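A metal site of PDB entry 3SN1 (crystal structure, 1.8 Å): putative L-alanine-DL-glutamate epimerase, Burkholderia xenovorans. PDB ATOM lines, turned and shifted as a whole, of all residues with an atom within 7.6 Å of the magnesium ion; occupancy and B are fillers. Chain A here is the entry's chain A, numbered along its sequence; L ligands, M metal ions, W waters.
Residues that only touch the magnesium ion: Lys 163 (3.9 Å) and Asn 221 (3.98 Å).
Within 4 Å of the magnesium ion: Lys 163, Asp 219, Asn 221, Glu 245 and Glu 269.
The side-chain carboxylate of Glu 343 is in salt-bridge range of the side-chain amino group of Lys 163, at 3.4 Å.
The indole nitrogen (NE1) of Trp 243 sits at hydrogen-bond distance from the side-chain carboxylate (OE2) of Glu 245 (2.9 Å).
The side-chain carboxylate (OE1) of Glu 269 sits close to a ring nitrogen (NE2) of His 318 (3.4 Å).
N of His 125 sits at hydrogen-bond distance from O of Lys 163.
OD2 of Asp 219 lies close to NZ of Lys 163.
The backbone NH of Asn 221 is in hydrogen-bond range of the side-chain carboxylate of Asp 219 (2.9 Å).
The backbone carbonyl oxygen of Glu 245 sits at hydrogen-bond distance from the backbone NH of Leu 220 (2.8 Å).
OD1 of Asn 221 sits at hydrogen-bond distance from ND2 of Asn 165.
Water W1 binds the magnesium ion (2.0 Å).
The side-chain carboxylate (OE1) of Glu 245 binds the magnesium ion (2.0 Å).
OE2 of Glu 269 binds the magnesium ion, 2.1 Å away.
The side-chain carboxylate (OD2) of Asp 219 binds the magnesium ion (2.1 Å).
An oxygen (O5) of the ligand is bound to the magnesium ion (2.2 Å).
O4 of the ligand is bound to the magnesium ion (2.2 Å).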
ATOM      1  N   PHE A  41      26.714 -24.542   4.198  1.00  0.00           N
ATOM      2  CA  PHE A  41      25.704 -25.326   3.494  1.00  0.00           C
ATOM      3  C   PHE A  41      25.786 -26.782   3.939  1.00  0.00           C
ATOM      4  O   PHE A  41      26.129 -27.687   3.160  1.00  0.00           O
ATOM      5  CB  PHE A  41      25.839 -25.148   1.995  1.00  0.00           C
ATOM      6  CG  PHE A  41      24.636 -25.610   1.207  1.00  0.00           C
ATOM      7  CD1 PHE A  41      23.337 -25.257   1.599  1.00  0.00           C
ATOM      8  CD2 PHE A  41      24.791 -26.368   0.070  1.00  0.00           C
ATOM      9  CE1 PHE A  41      22.240 -25.685   0.880  1.00  0.00           C
ATOM     10  CE2 PHE A  41      23.670 -26.782  -0.688  1.00  0.00           C
ATOM     11  CZ  PHE A  41      22.395 -26.443  -0.257  1.00  0.00           C
ATOM     12  N   TYR A 122      21.716 -16.562 -14.788  1.00  0.00           N
ATOM     13  CA  TYR A 122      20.538 -16.118 -14.077  1.00  0.00           C
ATOM     14  C   TYR A 122      20.933 -15.501 -12.744  1.00  0.00           C
ATOM     15  O   TYR A 122      21.902 -15.922 -12.097  1.00  0.00           O
ATOM     16  CB  TYR A 122      19.526 -17.236 -13.877  1.00  0.00           C
ATOM     17  CG  TYR A 122      19.920 -18.386 -13.005  1.00  0.00           C
ATOM     18  CD1 TYR A 122      19.583 -18.430 -11.655  1.00  0.00           C
ATOM     19  CD2 TYR A 122      20.561 -19.498 -13.541  1.00  0.00           C
ATOM     20  CE1 TYR A 122      19.911 -19.517 -10.859  1.00  0.00           C
ATOM     21  CE2 TYR A 122      20.884 -20.591 -12.752  1.00  0.00           C
ATOM     22  CZ  TYR A 122      20.544 -20.600 -11.415  1.00  0.00           C
ATOM     23  OH  TYR A 122      20.879 -21.689 -10.655  1.00  0.00           O
ATOM     24  N   SER A 124      20.395 -15.369  -9.229  1.00  0.00           N
ATOM     25  CA  SER A 124      19.895 -16.335  -8.278  1.00  0.00           C
ATOM     26  C   SER A 124      19.523 -15.659  -6.970  1.00  0.00           C
ATOM     27  O   SER A 124      19.882 -14.526  -6.728  1.00  0.00           O
ATOM     28  CB  SER A 124      20.941 -17.414  -8.077  1.00  0.00           C
ATOM     29  OG  SER A 124      20.339 -18.546  -7.504  1.00  0.00           O
ATOM     30  N   HIS A 125      18.807 -16.390  -6.119  1.00  0.00           N
ATOM     31  CA  HIS A 125      18.348 -15.880  -4.831  1.00  0.00           C
ATOM     32  C   HIS A 125      17.716 -14.519  -4.977  1.00  0.00           C
ATOM     33  O   HIS A 125      18.056 -13.579  -4.275  1.00  0.00           O
ATOM     34  CB  HIS A 125      19.507 -15.862  -3.846  1.00  0.00           C
ATOM     35  CG  HIS A 125      20.050 -17.225  -3.595  1.00  0.00           C
ATOM     36  ND1 HIS A 125      21.167 -17.721  -4.242  1.00  0.00           N
ATOM     37  CD2 HIS A 125      19.560 -18.261  -2.854  1.00  0.00           C
ATOM     38  CE1 HIS A 125      21.358 -18.972  -3.876  1.00  0.00           C
ATOM     39  NE2 HIS A 125      20.409 -19.319  -3.020  1.00  0.00           N
ATOM     40  N   LYS A 163      15.946 -16.472 -10.283  1.00  0.00           N
ATOM     41  CA  LYS A 163      15.518 -17.652  -9.532  1.00  0.00           C
ATOM     42  C   LYS A 163      15.104 -17.355  -8.116  1.00  0.00           C
ATOM     43  O   LYS A 163      15.870 -16.747  -7.357  1.00  0.00           O
ATOM     44  CB  LYS A 163      16.617 -18.704  -9.506  1.00  0.00           C
ATOM     45  CG  LYS A 163      16.167 -20.033  -8.904  1.00  0.00           C
ATOM     46  CD  LYS A 163      17.152 -21.191  -9.158  1.00  0.00           C
ATOM     47  CE  LYS A 163      18.266 -21.291  -8.113  1.00  0.00           C
ATOM     48  NZ  LYS A 163      19.313 -22.293  -8.504  1.00  0.00           N
ATOM     49  N   ASN A 165      12.702 -18.895  -4.484  1.00  0.00           N
ATOM     50  CA  ASN A 165      12.501 -20.061  -3.607  1.00  0.00           C
ATOM     51  C   ASN A 165      11.053 -20.020  -3.107  1.00  0.00           C
ATOM     52  O   ASN A 165      10.196 -19.534  -3.825  1.00  0.00           O
ATOM     53  CB  ASN A 165      13.541 -20.035  -2.469  1.00  0.00           C
ATOM     54  CG  ASN A 165      14.968 -20.109  -2.986  1.00  0.00           C
ATOM     55  OD1 ASN A 165      15.574 -19.085  -3.378  1.00  0.00           O
ATOM     56  ND2 ASN A 165      15.541 -21.314  -3.002  1.00  0.00           N
ATOM     57  N   LEU A 218      12.387 -21.634 -10.468  1.00  0.00           N
ATOM     58  CA  LEU A 218      11.874 -21.910  -9.101  1.00  0.00           C
ATOM     59  C   LEU A 218      12.687 -23.019  -8.452  1.00  0.00           C
ATOM     60  O   LEU A 218      12.788 -24.117  -8.993  1.00  0.00           O
ATOM     61  CB  LEU A 218      10.402 -22.311  -9.134  1.00  0.00           C
ATOM     62  CG  LEU A 218       9.694 -22.678  -7.824  1.00  0.00           C
ATOM     63  CD1 LEU A 218       9.712 -21.507  -6.840  1.00  0.00           C
ATOM     64  CD2 LEU A 218       8.276 -23.116  -8.086  1.00  0.00           C
ATOM     65  N   ASP A 219      13.281 -22.728  -7.298  1.00  0.00           N
ATOM     66  CA  ASP A 219      14.059 -23.704  -6.549  1.00  0.00           C
ATOM     67  C   ASP A 219      13.266 -24.157  -5.328  1.00  0.00           C
ATOM     68  O   ASP A 219      12.981 -23.365  -4.422  1.00  0.00           O
ATOM     69  CB  ASP A 219      15.400 -23.114  -6.105  1.00  0.00           C
ATOM     70  CG  ASP A 219      16.425 -24.191  -5.733  1.00  0.00           C
ATOM     71  OD1 ASP A 219      16.016 -25.348  -5.451  1.00  0.00           O
ATOM     72  OD2 ASP A 219      17.649 -23.886  -5.758  1.00  0.00           O
ATOM     73  N   LEU A 220      12.952 -25.450  -5.286  1.00  0.00           N
ATOM     74  CA  LEU A 220      12.245 -26.045  -4.155  1.00  0.00           C
ATOM     75  C   LEU A 220      13.154 -26.794  -3.180  1.00  0.00           C
ATOM     76  O   LEU A 220      12.676 -27.313  -2.161  1.00  0.00           O
ATOM     77  CB  LEU A 220      11.162 -27.001  -4.684  1.00  0.00           C
ATOM     78  CG  LEU A 220      10.164 -26.404  -5.674  1.00  0.00           C
ATOM     79  CD1 LEU A 220       9.195 -27.520  -6.160  1.00  0.00           C
ATOM     80  CD2 LEU A 220       9.386 -25.258  -5.054  1.00  0.00           C
ATOM     81  N   ASN A 221      14.447 -26.823  -3.486  1.00  0.00           N
ATOM     82  CA  ASN A 221      15.451 -27.467  -2.646  1.00  0.00           C
ATOM     83  C   ASN A 221      14.962 -28.868  -2.199  1.00  0.00           C
ATOM     84  O   ASN A 221      14.462 -29.624  -3.034  1.00  0.00           O
ATOM     85  CB  ASN A 221      15.864 -26.543  -1.496  1.00  0.00           C
ATOM     86  CG  ASN A 221      16.482 -25.260  -1.963  1.00  0.00           C
ATOM     87  OD1 ASN A 221      15.790 -24.262  -2.183  1.00  0.00           O
ATOM     88  ND2 ASN A 221      17.817 -25.265  -2.108  1.00  0.00           N
ATOM     89  N   TRP A 243      12.850 -23.565 -15.221  1.00  0.00           N
ATOM     90  CA  TRP A 243      12.994 -24.874 -14.597  1.00  0.00           C
ATOM     91  C   TRP A 243      12.436 -24.829 -13.203  1.00  0.00           C
ATOM     92  O   TRP A 243      12.249 -23.757 -12.632  1.00  0.00           O
ATOM     93  CB  TRP A 243      14.420 -25.420 -14.618  1.00  0.00           C
ATOM     94  CG  TRP A 243      15.474 -24.874 -13.625  1.00  0.00           C
ATOM     95  CD1 TRP A 243      15.312 -24.572 -12.310  1.00  0.00           C
ATOM     96  CD2 TRP A 243      16.870 -24.709 -13.902  1.00  0.00           C
ATOM     97  NE1 TRP A 243      16.520 -24.199 -11.744  1.00  0.00           N
ATOM     98  CE2 TRP A 243      17.488 -24.273 -12.705  1.00  0.00           C
ATOM     99  CE3 TRP A 243      17.656 -24.872 -15.040  1.00  0.00           C
ATOM    100  CZ2 TRP A 243      18.834 -24.006 -12.626  1.00  0.00           C
ATOM    101  CZ3 TRP A 243      19.002 -24.592 -14.957  1.00  0.00           C
ATOM    102  CH2 TRP A 243      19.579 -24.151 -13.762  1.00  0.00           C
ATOM    103  N   GLU A 245      13.547 -26.690  -9.700  1.00  0.00           N
ATOM    104  CA  GLU A 245      14.730 -27.322  -9.171  1.00  0.00           C
ATOM    105  C   GLU A 245      14.332 -28.074  -7.927  1.00  0.00           C
ATOM    106  O   GLU A 245      13.726 -27.514  -6.995  1.00  0.00           O
ATOM    107  CB  GLU A 245      15.750 -26.222  -8.853  1.00  0.00           C
ATOM    108  CG  GLU A 245      17.147 -26.629  -8.474  1.00  0.00           C
ATOM    109  CD  GLU A 245      18.120 -25.429  -8.481  1.00  0.00           C
ATOM    110  OE1 GLU A 245      19.123 -25.496  -7.759  1.00  0.00           O
ATOM    111  OE2 GLU A 245      17.884 -24.439  -9.223  1.00  0.00           O
ATOM    112  N   ILE A 246      14.644 -29.370  -7.916  1.00  0.00           N
ATOM    113  CA  ILE A 246      14.202 -30.280  -6.842  1.00  0.00           C
ATOM    114  C   ILE A 246      15.393 -31.167  -6.459  1.00  0.00           C
ATOM    115  O   ILE A 246      15.912 -31.924  -7.291  1.00  0.00           O
ATOM    116  CB  ILE A 246      13.045 -31.181  -7.310  1.00  0.00           C
ATOM    117  CG1 ILE A 246      11.820 -30.325  -7.639  1.00  0.00           C
ATOM    118  CG2 ILE A 246      12.718 -32.258  -6.235  1.00  0.00           C
ATOM    119  CD1 ILE A 246      10.653 -31.124  -8.295  1.00  0.00           C
ATOM    120  N   ASP A 247      15.852 -31.049  -5.217  1.00  0.00           N
ATOM    121  CA  ASP A 247      16.867 -31.937  -4.690  1.00  0.00           C
ATOM    122  C   ASP A 247      16.241 -33.169  -4.058  1.00  0.00           C
ATOM    123  O   ASP A 247      15.270 -33.067  -3.288  1.00  0.00           O
ATOM    124  CB  ASP A 247      17.735 -31.202  -3.689  1.00  0.00           C
ATOM    125  CG  ASP A 247      18.507 -30.084  -4.312  1.00  0.00           C
ATOM    126  OD1 ASP A 247      19.285 -30.351  -5.264  1.00  0.00           O
ATOM    127  OD2 ASP A 247      18.306 -28.941  -3.867  1.00  0.00           O
ATOM    128  N   SER A 266      15.374 -29.504 -12.884  1.00  0.00           N
ATOM    129  CA  SER A 266      16.788 -29.534 -12.592  1.00  0.00           C
ATOM    130  C   SER A 266      17.024 -30.120 -11.205  1.00  0.00           C
ATOM    131  O   SER A 266      16.151 -30.061 -10.324  1.00  0.00           O
ATOM    132  CB  SER A 266      17.403 -28.143 -12.655  1.00  0.00           C
ATOM    133  OG  SER A 266      16.811 -27.293 -11.703  1.00  0.00           O
ATOM    134  N   SER A 267      18.200 -30.717 -11.025  1.00  0.00           N
ATOM    135  CA  SER A 267      18.610 -31.271  -9.745  1.00  0.00           C
ATOM    136  C   SER A 267      20.123 -31.481  -9.737  1.00  0.00           C
ATOM    137  O   SER A 267      20.839 -31.162 -10.702  1.00  0.00           O
ATOM    138  CB  SER A 267      17.908 -32.622  -9.491  1.00  0.00           C
ATOM    139  OG  SER A 267      17.957 -33.080  -8.136  1.00  0.00           O
ATOM    140  N   CYS A 268      20.582 -32.024  -8.614  1.00  0.00           N
ATOM    141  CA  CYS A 268      21.884 -32.679  -8.457  1.00  0.00           C
ATOM    142  C   CYS A 268      22.953 -31.797  -7.839  1.00  0.00           C
ATOM    143  O   CYS A 268      24.114 -32.230  -7.771  1.00  0.00           O
ATOM    144  CB  CYS A 268      22.441 -33.254  -9.753  1.00  0.00           C
ATOM    145  SG  CYS A 268      21.316 -34.330 -10.687  1.00  0.00           S
ATOM    146  N   GLU A 269      22.604 -30.605  -7.391  1.00  0.00           N
ATOM    147  CA  GLU A 269      23.619 -29.667  -6.869  1.00  0.00           C
ATOM    148  C   GLU A 269      24.430 -30.217  -5.720  1.00  0.00           C
ATOM    149  O   GLU A 269      25.512 -29.685  -5.433  1.00  0.00           O
ATOM    150  CB  GLU A 269      23.022 -28.306  -6.455  1.00  0.00           C
ATOM    151  CG  GLU A 269      22.238 -28.331  -5.144  1.00  0.00           C
ATOM    152  CD  GLU A 269      21.476 -27.043  -4.889  1.00  0.00           C
ATOM    153  OE1 GLU A 269      21.300 -26.671  -3.699  1.00  0.00           O
ATOM    154  OE2 GLU A 269      21.071 -26.393  -5.884  1.00  0.00           O
ATOM    155  N   THR A 270      23.899 -31.228  -5.013  1.00  0.00           N
ATOM    156  CA  THR A 270      24.594 -31.778  -3.846  1.00  0.00           C
ATOM    157  C   THR A 270      25.347 -33.091  -4.119  1.00  0.00           C
ATOM    158  O   THR A 270      25.866 -33.696  -3.178  1.00  0.00           O
ATOM    159  CB  THR A 270      23.610 -32.056  -2.666  1.00  0.00           C
ATOM    160  OG1 THR A 270      22.722 -33.122  -3.028  1.00  0.00           O
ATOM    161  CG2 THR A 270      22.846 -30.765  -2.318  1.00  0.00           C
ATOM    162  N   ILE A 290      22.656 -29.958 -12.331  1.00  0.00           N
ATOM    163  CA  ILE A 290      23.406 -28.912 -11.669  1.00  0.00           C
ATOM    164  C   ILE A 290      24.640 -29.552 -11.051  1.00  0.00           C
ATOM    165  O   ILE A 290      24.537 -30.566 -10.352  1.00  0.00           O
ATOM    166  CB  ILE A 290      22.568 -28.216 -10.601  1.00  0.00           C
ATOM    167  CG1 ILE A 290      21.392 -27.471 -11.261  1.00  0.00           C
ATOM    168  CG2 ILE A 290      23.422 -27.204  -9.809  1.00  0.00           C
ATOM    169  CD1 ILE A 290      20.225 -27.265 -10.327  1.00  0.00           C
ATOM    170  N   HIS A 318      26.662 -24.825  -9.858  1.00  0.00           N
ATOM    171  CA  HIS A 318      26.052 -24.393  -8.613  1.00  0.00           C
ATOM    172  C   HIS A 318      26.976 -23.304  -8.067  1.00  0.00           C
ATOM    173  O   HIS A 318      28.121 -23.573  -7.739  1.00  0.00           O
ATOM    174  CB  HIS A 318      26.002 -25.578  -7.656  1.00  0.00           C
ATOM    175  CG  HIS A 318      25.263 -25.312  -6.381  1.00  0.00           C
ATOM    176  ND1 HIS A 318      25.648 -25.891  -5.198  1.00  0.00           N
ATOM    177  CD2 HIS A 318      24.135 -24.609  -6.118  1.00  0.00           C
ATOM    178  CE1 HIS A 318      24.822 -25.518  -4.236  1.00  0.00           C
ATOM    179  NE2 HIS A 318      23.890 -24.746  -4.765  1.00  0.00           N
ATOM    180  N   PHE A 320      26.777 -19.843  -5.635  1.00  0.00           N
ATOM    181  CA  PHE A 320      26.088 -18.903  -4.757  1.00  0.00           C
ATOM    182  C   PHE A 320      26.950 -18.478  -3.565  1.00  0.00           C
ATOM    183  O   PHE A 320      26.482 -18.306  -2.447  1.00  0.00           O
ATOM    184  CB  PHE A 320      24.722 -19.468  -4.303  1.00  0.00           C
ATOM    185  CG  PHE A 320      24.779 -20.499  -3.195  1.00  0.00           C
ATOM    186  CD1 PHE A 320      24.203 -20.221  -1.939  1.00  0.00           C
ATOM    187  CD2 PHE A 320      25.324 -21.747  -3.399  1.00  0.00           C
ATOM    188  CE1 PHE A 320      24.222 -21.168  -0.917  1.00  0.00           C
ATOM    189  CE2 PHE A 320      25.354 -22.696  -2.369  1.00  0.00           C
ATOM    190  CZ  PHE A 320      24.807 -22.413  -1.141  1.00  0.00           C
ATOM    191  N   GLU A 343      24.600 -19.958 -12.851  1.00  0.00           N
ATOM    192  CA  GLU A 343      24.025 -19.328 -11.678  1.00  0.00           C
ATOM    193  C   GLU A 343      24.974 -18.285 -11.146  1.00  0.00           C
ATOM    194  O   GLU A 343      26.192 -18.497 -11.111  1.00  0.00           O
ATOM    195  CB  GLU A 343      23.836 -20.385 -10.610  1.00  0.00           C
ATOM    196  CG  GLU A 343      23.240 -19.830  -9.326  1.00  0.00           C
ATOM    197  CD  GLU A 343      22.946 -20.872  -8.277  1.00  0.00           C
ATOM    198  OE1 GLU A 343      23.584 -21.939  -8.263  1.00  0.00           O
ATOM    199  OE2 GLU A 343      22.071 -20.586  -7.432  1.00  0.00           O
HETATM  200  O1  LIG L   1      20.827 -23.352  -0.459  1.00  0.00           O
HETATM  201  O2  LIG L   1      20.113 -21.466  -1.370  1.00  0.00           O
HETATM  202  C1  LIG L   1      20.765 -22.549  -1.431  1.00  0.00           C
HETATM  203  C2  LIG L   1      21.479 -22.889  -2.716  1.00  0.00           C
HETATM  204  O3  LIG L   1      22.301 -24.056  -2.566  1.00  0.00           O
HETATM  205  C3  LIG L   1      20.462 -23.086  -3.820  1.00  0.00           C
HETATM  206  O4  LIG L   1      19.930 -24.415  -3.786  1.00  0.00           O
HETATM  207  C4  LIG L   1      21.048 -22.787  -5.173  1.00  0.00           C
HETATM  208  O5  LIG L   1      20.588 -23.384  -6.175  1.00  0.00           O
HETATM  209  O6  LIG L   1      21.898 -21.874  -5.268  1.00  0.00           O
HETATM  210 MG    MG M   1      19.387 -25.127  -5.768  1.00  0.00          MG
HETATM  211  O   HOH W   1      18.237 -26.664  -5.098  1.00  0.00           O
